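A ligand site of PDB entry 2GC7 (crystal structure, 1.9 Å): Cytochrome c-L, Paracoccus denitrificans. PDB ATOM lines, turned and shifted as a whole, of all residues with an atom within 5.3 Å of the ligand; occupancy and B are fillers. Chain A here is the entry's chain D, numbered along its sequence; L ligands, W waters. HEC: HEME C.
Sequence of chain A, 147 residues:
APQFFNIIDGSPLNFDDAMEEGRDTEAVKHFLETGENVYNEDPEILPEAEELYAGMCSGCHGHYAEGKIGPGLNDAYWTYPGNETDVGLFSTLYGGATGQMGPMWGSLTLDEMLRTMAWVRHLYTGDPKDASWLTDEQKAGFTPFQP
The backbone carbonyl oxygen (O) of Tyr 80 sits close to the side-chain amide nitrogen (ND2) of Asn 83.
O of Leu 93 lies within hydrogen-bond range of N of Met 104 (2.9 Å).
The side-chain amide oxygen (OD1) of Asn 83 lies within hydrogen-bond range of the backbone NH (N) of Leu 89.
A ring nitrogen (ND1) of His 61 is in hydrogen-bond range of the backbone carbonyl oxygen (O) of Pro 71 (2.5 Å).
The side-chain amide oxygen (OD1) of Asn 83 sits at hydrogen-bond distance from the side-chain hydroxyl (OG1) of Thr 92, 2.8 Å away.
The backbone NH of Gly 70 sits at hydrogen-bond distance from the backbone carbonyl oxygen of Cys 60, 2.8 Å away.
The backbone NH (N) of Ile 69 sits at hydrogen-bond distance from the backbone carbonyl oxygen (O) of Cys 60, at 3.3 Å.
O of Met 56 touches CMC of the ligand, 3.2 Å away.
Pro 71 touches the ligand.
CD2 of Leu 73 touches C3A of the ligand, 3.7 Å away.
Trp 78 touches the ligand.
Leu 89 touches the ligand (CD2 to CMA, 3.6 Å).
Leu 93 touches the ligand.
Ala 97 touches the ligand (CB to O1D, 3.6 Å).
CB of Gln 100 touches CBC of the ligand (3.6 Å).
Met 104 touches the ligand (SD to CBB, 3.7 Å).
Thr 116 touches the ligand (CG2 to CMB, 3.96 Å).
CG2 of Val 120 touches CMB of the ligand (3.99 Å).
Hydrophobic or aromatic side chains within 4 Å of the ligand: Met 56, His 61, Pro 71, Leu 73, Trp 78, Tyr 80, Leu 89, Leu 93, Ala 97, Met 101, Met 104 and Val 120.
Of the 27 residues printed, 19 come within 4 Å of the ligand.
SG of Cys 60 is bonded to CAC of the ligand, at 1.8 Å.
An oxygen (O1D) of the ligand sits at hydrogen-bond distance from the backbone NH (N) of Thr 98, 3.4 Å away.
NE2 of His 61 is bound to FE of the ligand (2.0 Å).
The side-chain hydroxyl (OG1) of Thr 98 sits at hydrogen-bond distance from an oxygen (O1D) of the ligand.
A carbon (CAB) of the ligand is covalently linked to the side-chain sulfur (SG) of Cys 57 (1.7 Å).
The side-chain sulfur (SD) of Met 101 is bound to an iron atom (FE) of the ligand (2.3 Å).
O2A of the ligand lies within hydrogen-bond range of N of Thr 79, at 2.7 Å.
ND2 of Asn 83 lies within hydrogen-bond range of O1A of the ligand (2.8 Å).
N of Tyr 80 is in hydrogen-bond range of O1A of the ligand (3.0 Å).
An oxygen (O1D) of the ligand lies within hydrogen-bond range of the side-chain hydroxyl (OH) of Tyr 80, 2.6 Å away.
OG1 of Thr 79 is in hydrogen-bond range of O2A of the ligand, at 3.3 Å.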
ATOM      1  N   ILE A   8      -3.665   9.174   2.460  1.00  0.00           N
ATOM      2  CA  ILE A   8      -4.080   8.905   3.827  1.00  0.00           C
ATOM      3  C   ILE A   8      -4.271  10.165   4.670  1.00  0.00           C
ATOM      4  O   ILE A   8      -5.303  10.341   5.304  1.00  0.00           O
ATOM      5  CB  ILE A   8      -3.075   7.986   4.546  1.00  0.00           C
ATOM      6  CG1 ILE A   8      -2.964   6.657   3.796  1.00  0.00           C
ATOM      7  CG2 ILE A   8      -3.525   7.747   5.981  1.00  0.00           C
ATOM      8  CD1 ILE A   8      -4.268   5.886   3.700  1.00  0.00           C
ATOM      9  N   TYR A  53       6.060  -5.554 -12.067  1.00  0.00           N
ATOM     10  CA  TYR A  53       4.972  -5.968 -11.183  1.00  0.00           C
ATOM     11  C   TYR A  53       5.285  -7.321 -10.544  1.00  0.00           C
ATOM     12  O   TYR A  53       5.064  -7.521  -9.350  1.00  0.00           O
ATOM     13  CB  TYR A  53       3.660  -6.067 -11.968  1.00  0.00           C
ATOM     14  CG  TYR A  53       2.513  -6.590 -11.139  1.00  0.00           C
ATOM     15  CD1 TYR A  53       1.762  -5.736 -10.343  1.00  0.00           C
ATOM     16  CD2 TYR A  53       2.222  -7.958 -11.104  1.00  0.00           C
ATOM     17  CE1 TYR A  53       0.742  -6.230  -9.516  1.00  0.00           C
ATOM     18  CE2 TYR A  53       1.218  -8.452 -10.290  1.00  0.00           C
ATOM     19  CZ  TYR A  53       0.475  -7.588  -9.500  1.00  0.00           C
ATOM     20  OH  TYR A  53      -0.496  -8.092  -8.662  1.00  0.00           O
ATOM     21  N   MET A  56       8.013  -6.875  -7.735  1.00  0.00           N
ATOM     22  CA  MET A  56       7.648  -5.954  -6.661  1.00  0.00           C
ATOM     23  C   MET A  56       6.249  -6.035  -6.062  1.00  0.00           C
ATOM     24  O   MET A  56       6.039  -5.595  -4.938  1.00  0.00           O
ATOM     25  CB  MET A  56       7.854  -4.515  -7.145  1.00  0.00           C
ATOM     26  CG  MET A  56       9.297  -4.145  -7.427  1.00  0.00           C
ATOM     27  SD  MET A  56      10.008  -3.292  -6.023  1.00  0.00           S
ATOM     28  CE  MET A  56      10.210  -4.606  -4.876  1.00  0.00           C
ATOM     29  N   CYS A  57       5.284  -6.597  -6.800  1.00  0.00           N
ATOM     30  CA  CYS A  57       3.908  -6.618  -6.298  1.00  0.00           C
ATOM     31  C   CYS A  57       3.181  -7.953  -6.226  1.00  0.00           C
ATOM     32  O   CYS A  57       2.285  -8.117  -5.395  1.00  0.00           O
ATOM     33  CB  CYS A  57       3.060  -5.690  -7.173  1.00  0.00           C
ATOM     34  SG  CYS A  57       3.940  -4.265  -7.877  1.00  0.00           S
ATOM     35  N   CYS A  60       2.321 -10.062  -2.921  1.00  0.00           N
ATOM     36  CA  CYS A  60       1.232  -9.675  -2.044  1.00  0.00           C
ATOM     37  C   CYS A  60      -0.131  -9.554  -2.719  1.00  0.00           C
ATOM     38  O   CYS A  60      -1.149  -9.908  -2.127  1.00  0.00           O
ATOM     39  CB  CYS A  60       1.531  -8.348  -1.347  1.00  0.00           C
ATOM     40  SG  CYS A  60       2.918  -8.390  -0.171  1.00  0.00           S
ATOM     41  N   HIS A  61      -0.146  -9.052  -3.949  1.00  0.00           N
ATOM     42  CA  HIS A  61      -1.382  -8.832  -4.677  1.00  0.00           C
ATOM     43  C   HIS A  61      -1.788  -9.937  -5.661  1.00  0.00           C
ATOM     44  O   HIS A  61      -2.836  -9.849  -6.285  1.00  0.00           O
ATOM     45  CB  HIS A  61      -1.319  -7.481  -5.394  1.00  0.00           C
ATOM     46  CG  HIS A  61      -1.414  -6.312  -4.450  1.00  0.00           C
ATOM     47  ND1 HIS A  61      -2.569  -6.045  -3.778  1.00  0.00           N
ATOM     48  CD2 HIS A  61      -0.318  -5.540  -4.261  1.00  0.00           C
ATOM     49  CE1 HIS A  61      -2.177  -4.959  -3.030  1.00  0.00           C
ATOM     50  NE2 HIS A  61      -0.813  -4.638  -3.312  1.00  0.00           N
ATOM     51  N   ILE A  69      -2.469 -12.161  -0.130  1.00  0.00           N
ATOM     52  CA  ILE A  69      -2.422 -11.754   1.274  1.00  0.00           C
ATOM     53  C   ILE A  69      -2.748 -10.271   1.308  1.00  0.00           C
ATOM     54  O   ILE A  69      -3.007  -9.701   2.371  1.00  0.00           O
ATOM     55  CB  ILE A  69      -1.053 -12.005   1.957  1.00  0.00           C
ATOM     56  CG1 ILE A  69       0.051 -11.162   1.309  1.00  0.00           C
ATOM     57  CG2 ILE A  69      -0.696 -13.487   1.897  1.00  0.00           C
ATOM     58  CD1 ILE A  69       0.633 -11.784   0.071  1.00  0.00           C
ATOM     59  N   GLY A  70      -2.738  -9.660   0.124  1.00  0.00           N
ATOM     60  CA  GLY A  70      -3.061  -8.257  -0.026  1.00  0.00           C
ATOM     61  C   GLY A  70      -4.300  -8.207  -0.896  1.00  0.00           C
ATOM     62  O   GLY A  70      -4.623  -9.213  -1.532  1.00  0.00           O
ATOM     63  N   PRO A  71      -5.009  -7.071  -0.963  1.00  0.00           N
ATOM     64  CA  PRO A  71      -6.232  -6.921  -1.767  1.00  0.00           C
ATOM     65  C   PRO A  71      -6.074  -6.970  -3.286  1.00  0.00           C
ATOM     66  O   PRO A  71      -5.040  -6.557  -3.827  1.00  0.00           O
ATOM     67  CB  PRO A  71      -6.785  -5.578  -1.300  1.00  0.00           C
ATOM     68  CG  PRO A  71      -5.539  -4.807  -1.039  1.00  0.00           C
ATOM     69  CD  PRO A  71      -4.680  -5.805  -0.291  1.00  0.00           C
ATOM     70  N   GLY A  72      -7.101  -7.482  -3.959  1.00  0.00           N
ATOM     71  CA  GLY A  72      -7.071  -7.559  -5.413  1.00  0.00           C
ATOM     72  C   GLY A  72      -7.039  -6.159  -6.012  1.00  0.00           C
ATOM     73  O   GLY A  72      -7.469  -5.207  -5.377  1.00  0.00           O
ATOM     74  N   LEU A  73      -6.526  -6.041  -7.228  1.00  0.00           N
ATOM     75  CA  LEU A  73      -6.433  -4.740  -7.878  1.00  0.00           C
ATOM     76  C   LEU A  73      -6.960  -4.814  -9.299  1.00  0.00           C
ATOM     77  O   LEU A  73      -6.751  -3.894 -10.088  1.00  0.00           O
ATOM     78  CB  LEU A  73      -4.967  -4.281  -7.945  1.00  0.00           C
ATOM     79  CG  LEU A  73      -4.086  -4.409  -6.690  1.00  0.00           C
ATOM     80  CD1 LEU A  73      -2.642  -4.139  -7.065  1.00  0.00           C
ATOM     81  CD2 LEU A  73      -4.556  -3.447  -5.619  1.00  0.00           C
ATOM     82  N   TYR A  77     -13.652  -2.118  -7.948  1.00  0.00           N
ATOM     83  CA  TYR A  77     -13.703  -1.689  -6.553  1.00  0.00           C
ATOM     84  C   TYR A  77     -12.334  -1.250  -6.047  1.00  0.00           C
ATOM     85  O   TYR A  77     -11.323  -1.937  -6.279  1.00  0.00           O
ATOM     86  CB  TYR A  77     -14.217  -2.807  -5.630  1.00  0.00           C
ATOM     87  CG  TYR A  77     -14.167  -2.380  -4.176  1.00  0.00           C
ATOM     88  CD1 TYR A  77     -15.096  -1.484  -3.673  1.00  0.00           C
ATOM     89  CD2 TYR A  77     -13.134  -2.799  -3.347  1.00  0.00           C
ATOM     90  CE1 TYR A  77     -14.996  -0.997  -2.364  1.00  0.00           C
ATOM     91  CE2 TYR A  77     -13.012  -2.322  -2.042  1.00  0.00           C
ATOM     92  CZ  TYR A  77     -13.953  -1.415  -1.555  1.00  0.00           C
ATOM     93  OH  TYR A  77     -13.843  -0.928  -0.280  1.00  0.00           O
ATOM     94  N   TRP A  78     -12.292  -0.122  -5.346  1.00  0.00           N
ATOM     95  CA  TRP A  78     -11.056   0.399  -4.781  1.00  0.00           C
ATOM     96  C   TRP A  78     -11.295   0.868  -3.347  1.00  0.00           C
ATOM     97  O   TRP A  78     -12.230   1.625  -3.087  1.00  0.00           O
ATOM     98  CB  TRP A  78     -10.516   1.566  -5.595  1.00  0.00           C
ATOM     99  CG  TRP A  78     -10.178   1.246  -7.020  1.00  0.00           C
ATOM    100  CD1 TRP A  78     -10.960   1.463  -8.123  1.00  0.00           C
ATOM    101  CD2 TRP A  78      -8.972   0.638  -7.503  1.00  0.00           C
ATOM    102  NE1 TRP A  78     -10.308   1.030  -9.263  1.00  0.00           N
ATOM    103  CE2 TRP A  78      -9.088   0.521  -8.913  1.00  0.00           C
ATOM    104  CE3 TRP A  78      -7.798   0.178  -6.881  1.00  0.00           C
ATOM    105  CZ2 TRP A  78      -8.072  -0.025  -9.705  1.00  0.00           C
ATOM    106  CZ3 TRP A  78      -6.789  -0.368  -7.681  1.00  0.00           C
ATOM    107  CH2 TRP A  78      -6.942  -0.464  -9.073  1.00  0.00           C
ATOM    108  N   THR A  79     -10.448   0.431  -2.429  1.00  0.00           N
ATOM    109  CA  THR A  79     -10.548   0.829  -1.032  1.00  0.00           C
ATOM    110  C   THR A  79     -10.413   2.348  -0.990  1.00  0.00           C
ATOM    111  O   THR A  79     -11.097   3.032  -0.237  1.00  0.00           O
ATOM    112  CB  THR A  79      -9.440   0.190  -0.189  1.00  0.00           C
ATOM    113  OG1 THR A  79      -9.629  -1.229  -0.173  1.00  0.00           O
ATOM    114  CG2 THR A  79      -9.456   0.728   1.230  1.00  0.00           C
ATOM    115  N   TYR A  80      -9.508   2.853  -1.813  1.00  0.00           N
ATOM    116  CA  TYR A  80      -9.268   4.281  -1.909  1.00  0.00           C
ATOM    117  C   TYR A  80      -9.825   4.647  -3.276  1.00  0.00           C
ATOM    118  O   TYR A  80      -9.197   4.385  -4.303  1.00  0.00           O
ATOM    119  CB  TYR A  80      -7.763   4.550  -1.802  1.00  0.00           C
ATOM    120  CG  TYR A  80      -7.204   4.094  -0.464  1.00  0.00           C
ATOM    121  CD1 TYR A  80      -7.430   4.834   0.701  1.00  0.00           C
ATOM    122  CD2 TYR A  80      -6.513   2.889  -0.357  1.00  0.00           C
ATOM    123  CE1 TYR A  80      -6.968   4.389   1.938  1.00  0.00           C
ATOM    124  CE2 TYR A  80      -6.051   2.434   0.879  1.00  0.00           C
ATOM    125  CZ  TYR A  80      -6.281   3.193   2.023  1.00  0.00           C
ATOM    126  OH  TYR A  80      -5.840   2.748   3.250  1.00  0.00           O
ATOM    127  N   ASN A  83      -8.209   5.801  -6.680  1.00  0.00           N
ATOM    128  CA  ASN A  83      -7.393   4.906  -7.492  1.00  0.00           C
ATOM    129  C   ASN A  83      -7.986   4.513  -8.834  1.00  0.00           C
ATOM    130  O   ASN A  83      -7.348   3.809  -9.626  1.00  0.00           O
ATOM    131  CB  ASN A  83      -7.003   3.662  -6.682  1.00  0.00           C
ATOM    132  CG  ASN A  83      -5.971   3.973  -5.625  1.00  0.00           C
ATOM    133  OD1 ASN A  83      -5.166   4.888  -5.804  1.00  0.00           O
ATOM    134  ND2 ASN A  83      -5.973   3.221  -4.539  1.00  0.00           N
ATOM    135  N   LEU A  89      -3.811   6.532  -8.366  1.00  0.00           N
ATOM    136  CA  LEU A  89      -3.014   5.316  -8.320  1.00  0.00           C
ATOM    137  C   LEU A  89      -1.559   5.685  -8.054  1.00  0.00           C
ATOM    138  O   LEU A  89      -0.883   5.089  -7.217  1.00  0.00           O
ATOM    139  CB  LEU A  89      -3.098   4.589  -9.671  1.00  0.00           C
ATOM    140  CG  LEU A  89      -3.051   3.058  -9.682  1.00  0.00           C
ATOM    141  CD1 LEU A  89      -2.557   2.607 -11.042  1.00  0.00           C
ATOM    142  CD2 LEU A  89      -2.158   2.530  -8.583  1.00  0.00           C
ATOM    143  N   THR A  92      -0.908   6.695  -4.497  1.00  0.00           N
ATOM    144  CA  THR A  92      -0.875   5.563  -3.586  1.00  0.00           C
ATOM    145  C   THR A  92       0.511   4.933  -3.569  1.00  0.00           C
ATOM    146  O   THR A  92       1.054   4.657  -2.502  1.00  0.00           O
ATOM    147  CB  THR A  92      -1.923   4.521  -3.999  1.00  0.00           C
ATOM    148  OG1 THR A  92      -3.233   5.091  -3.845  1.00  0.00           O
ATOM    149  CG2 THR A  92      -1.809   3.269  -3.130  1.00  0.00           C
ATOM    150  N   LEU A  93       1.090   4.711  -4.751  1.00  0.00           N
ATOM    151  CA  LEU A  93       2.421   4.121  -4.831  1.00  0.00           C
ATOM    152  C   LEU A  93       3.495   5.042  -4.246  1.00  0.00           C
ATOM    153  O   LEU A  93       4.303   4.615  -3.438  1.00  0.00           O
ATOM    154  CB  LEU A  93       2.791   3.811  -6.281  1.00  0.00           C
ATOM    155  CG  LEU A  93       1.982   2.718  -6.983  1.00  0.00           C
ATOM    156  CD1 LEU A  93       2.586   2.435  -8.354  1.00  0.00           C
ATOM    157  CD2 LEU A  93       2.000   1.466  -6.138  1.00  0.00           C
ATOM    158  N   ALA A  97       0.151   3.648   1.417  1.00  0.00           N
ATOM    159  CA  ALA A  97      -1.148   3.566   2.075  1.00  0.00           C
ATOM    160  C   ALA A  97      -0.863   3.242   3.537  1.00  0.00           C
ATOM    161  O   ALA A  97      -0.117   3.965   4.198  1.00  0.00           O
ATOM    162  CB  ALA A  97      -2.005   2.463   1.439  1.00  0.00           C
ATOM    163  N   THR A  98      -1.445   2.165   4.049  1.00  0.00           N
ATOM    164  CA  THR A  98      -1.195   1.781   5.436  1.00  0.00           C
ATOM    165  C   THR A  98      -0.586   0.377   5.493  1.00  0.00           C
ATOM    166  O   THR A  98      -0.545  -0.332   4.480  1.00  0.00           O
ATOM    167  CB  THR A  98      -2.488   1.769   6.258  1.00  0.00           C
ATOM    168  OG1 THR A  98      -3.330   0.686   5.844  1.00  0.00           O
ATOM    169  CG2 THR A  98      -3.242   3.075   6.075  1.00  0.00           C
ATOM    170  N   GLN A 100       1.783  -2.700   5.366  1.00  0.00           N
ATOM    171  CA  GLN A 100       2.929  -3.057   4.558  1.00  0.00           C
ATOM    172  C   GLN A 100       2.957  -2.386   3.190  1.00  0.00           C
ATOM    173  O   GLN A 100       3.922  -2.521   2.443  1.00  0.00           O
ATOM    174  CB  GLN A 100       3.017  -4.578   4.408  1.00  0.00           C
ATOM    175  CG  GLN A 100       3.554  -5.274   5.659  1.00  0.00           C
ATOM    176  CD  GLN A 100       3.621  -6.784   5.515  1.00  0.00           C
ATOM    177  OE1 GLN A 100       2.593  -7.467   5.516  1.00  0.00           O
ATOM    178  NE2 GLN A 100       4.829  -7.313   5.394  1.00  0.00           N
ATOM    179  N   MET A 101       1.893  -1.657   2.856  1.00  0.00           N
ATOM    180  CA  MET A 101       1.840  -0.935   1.594  1.00  0.00           C
ATOM    181  C   MET A 101       2.396   0.471   1.833  1.00  0.00           C
ATOM    182  O   MET A 101       1.656   1.436   1.998  1.00  0.00           O
ATOM    183  CB  MET A 101       0.404  -0.834   1.096  1.00  0.00           C
ATOM    184  CG  MET A 101       0.270  -0.221  -0.294  1.00  0.00           C
ATOM    185  SD  MET A 101       1.157  -1.155  -1.567  1.00  0.00           S
ATOM    186  CE  MET A 101       1.482   0.165  -2.722  1.00  0.00           C
ATOM    187  N   MET A 104       6.875   3.965  -2.286  1.00  0.00           N
ATOM    188  CA  MET A 104       7.746   3.270  -3.220  1.00  0.00           C
ATOM    189  C   MET A 104       8.818   4.173  -3.814  1.00  0.00           C
ATOM    190  O   MET A 104       9.578   3.739  -4.680  1.00  0.00           O
ATOM    191  CB  MET A 104       6.928   2.698  -4.378  1.00  0.00           C
ATOM    192  CG  MET A 104       5.799   1.755  -4.009  1.00  0.00           C
ATOM    193  SD  MET A 104       6.345   0.061  -3.824  1.00  0.00           S
ATOM    194  CE  MET A 104       5.323  -0.464  -2.451  1.00  0.00           C
ATOM    195  N   LEU A 108      11.467   2.628  -6.562  1.00  0.00           N
ATOM    196  CA  LEU A 108      11.119   2.803  -7.973  1.00  0.00           C
ATOM    197  C   LEU A 108      11.300   4.242  -8.423  1.00  0.00           C
ATOM    198  O   LEU A 108      11.022   5.173  -7.667  1.00  0.00           O
ATOM    199  CB  LEU A 108       9.654   2.404  -8.218  1.00  0.00           C
ATOM    200  CG  LEU A 108       9.221   0.947  -8.026  1.00  0.00           C
ATOM    201  CD1 LEU A 108       7.708   0.868  -8.034  1.00  0.00           C
ATOM    202  CD2 LEU A 108       9.815   0.084  -9.121  1.00  0.00           C
ATOM    203  N   THR A 116       4.773   0.398 -14.058  1.00  0.00           N
ATOM    204  CA  THR A 116       4.156  -0.599 -13.180  1.00  0.00           C
ATOM    205  C   THR A 116       2.652  -0.368 -13.180  1.00  0.00           C
ATOM    206  O   THR A 116       1.863  -1.312 -13.248  1.00  0.00           O
ATOM    207  CB  THR A 116       4.704  -0.485 -11.750  1.00  0.00           C
ATOM    208  OG1 THR A 116       6.109  -0.735 -11.760  1.00  0.00           O
ATOM    209  CG2 THR A 116       4.027  -1.491 -10.835  1.00  0.00           C
ATOM    210  N   VAL A 120      -0.825  -2.791 -14.072  1.00  0.00           N
ATOM    211  CA  VAL A 120      -1.976  -2.954 -13.187  1.00  0.00           C
ATOM    212  C   VAL A 120      -3.255  -2.654 -13.982  1.00  0.00           C
ATOM    213  O   VAL A 120      -4.252  -3.357 -13.864  1.00  0.00           O
ATOM    214  CB  VAL A 120      -1.886  -2.017 -11.956  1.00  0.00           C
ATOM    215  CG1 VAL A 120      -3.216  -1.988 -11.194  1.00  0.00           C
ATOM    216  CG2 VAL A 120      -0.763  -2.496 -11.033  1.00  0.00           C
HETATM  217 FE   HEC L   1      -0.001  -2.985  -2.453  1.00  0.00          FE
HETATM  218  CHA HEC L   1      -2.910  -1.796  -1.271  1.00  0.00           C
HETATM  219  CHB HEC L   1      -0.578  -1.376  -5.390  1.00  0.00           C
HETATM  220  CHC HEC L   1       3.021  -3.985  -3.624  1.00  0.00           C
HETATM  221  CHD HEC L   1       0.455  -4.883   0.309  1.00  0.00           C
HETATM  222  NA  HEC L   1      -1.471  -1.763  -3.187  1.00  0.00           N
HETATM  223  C1A HEC L   1      -2.596  -1.376  -2.526  1.00  0.00           C
HETATM  224  C2A HEC L   1      -3.377  -0.489  -3.366  1.00  0.00           C
HETATM  225  C3A HEC L   1      -2.710  -0.382  -4.553  1.00  0.00           C
HETATM  226  C4A HEC L   1      -1.519  -1.191  -4.441  1.00  0.00           C
HETATM  227  CMA HEC L   1      -3.116   0.453  -5.820  1.00  0.00           C
HETATM  228  CAA HEC L   1      -4.725   0.190  -2.947  1.00  0.00           C
HETATM  229  CBA HEC L   1      -5.911  -0.701  -3.400  1.00  0.00           C
HETATM  230  CGA HEC L   1      -7.295  -0.141  -3.211  1.00  0.00           C
HETATM  231  O1A HEC L   1      -7.420   1.160  -3.215  1.00  0.00           O
HETATM  232  O2A HEC L   1      -8.186  -0.935  -3.090  1.00  0.00           O
HETATM  233  NB  HEC L   1       1.016  -2.750  -4.175  1.00  0.00           N
HETATM  234  C1B HEC L   1       0.596  -2.065  -5.315  1.00  0.00           C
HETATM  235  C2B HEC L   1       1.584  -2.171  -6.379  1.00  0.00           C
HETATM  236  C3B HEC L   1       2.650  -2.859  -5.838  1.00  0.00           C
HETATM  237  C4B HEC L   1       2.272  -3.229  -4.504  1.00  0.00           C
HETATM  238  CMB HEC L   1       1.442  -1.567  -7.841  1.00  0.00           C
HETATM  239  CAB HEC L   1       4.016  -3.218  -6.491  1.00  0.00           C
HETATM  240  CBB HEC L   1       4.926  -1.944  -6.624  1.00  0.00           C
HETATM  241  NC  HEC L   1       1.473  -4.177  -1.760  1.00  0.00           N
HETATM  242  C1C HEC L   1       2.652  -4.455  -2.388  1.00  0.00           C
HETATM  243  C2C HEC L   1       3.446  -5.382  -1.610  1.00  0.00           C
HETATM  244  C3C HEC L   1       2.702  -5.688  -0.530  1.00  0.00           C
HETATM  245  C4C HEC L   1       1.474  -4.919  -0.624  1.00  0.00           C
HETATM  246  CMC HEC L   1       4.874  -5.931  -2.030  1.00  0.00           C
HETATM  247  CAC HEC L   1       2.977  -6.722   0.610  1.00  0.00           C
HETATM  248  CBC HEC L   1       4.172  -6.462   1.519  1.00  0.00           C
HETATM  249  ND  HEC L   1      -1.027  -3.270  -0.789  1.00  0.00           N
HETATM  250  C1D HEC L   1      -0.702  -4.114   0.286  1.00  0.00           C
HETATM  251  C2D HEC L   1      -1.709  -4.059   1.327  1.00  0.00           C
HETATM  252  C3D HEC L   1      -2.642  -3.161   0.898  1.00  0.00           C
HETATM  253  C4D HEC L   1      -2.215  -2.702  -0.425  1.00  0.00           C
HETATM  254  CMD HEC L   1      -1.696  -4.911   2.698  1.00  0.00           C
HETATM  255  CAD HEC L   1      -3.922  -2.683   1.623  1.00  0.00           C
HETATM  256  CBD HEC L   1      -3.586  -1.247   2.238  1.00  0.00           C
HETATM  257  CGD HEC L   1      -4.668  -0.490   2.932  1.00  0.00           C
HETATM  258  O1D HEC L   1      -4.370   0.617   3.395  1.00  0.00           O
HETATM  259  O2D HEC L   1      -5.810  -0.962   2.952  1.00  0.00           O
HETATM  260  O   HOH W   1      -0.142  -4.637   5.736  1.00  0.00           O
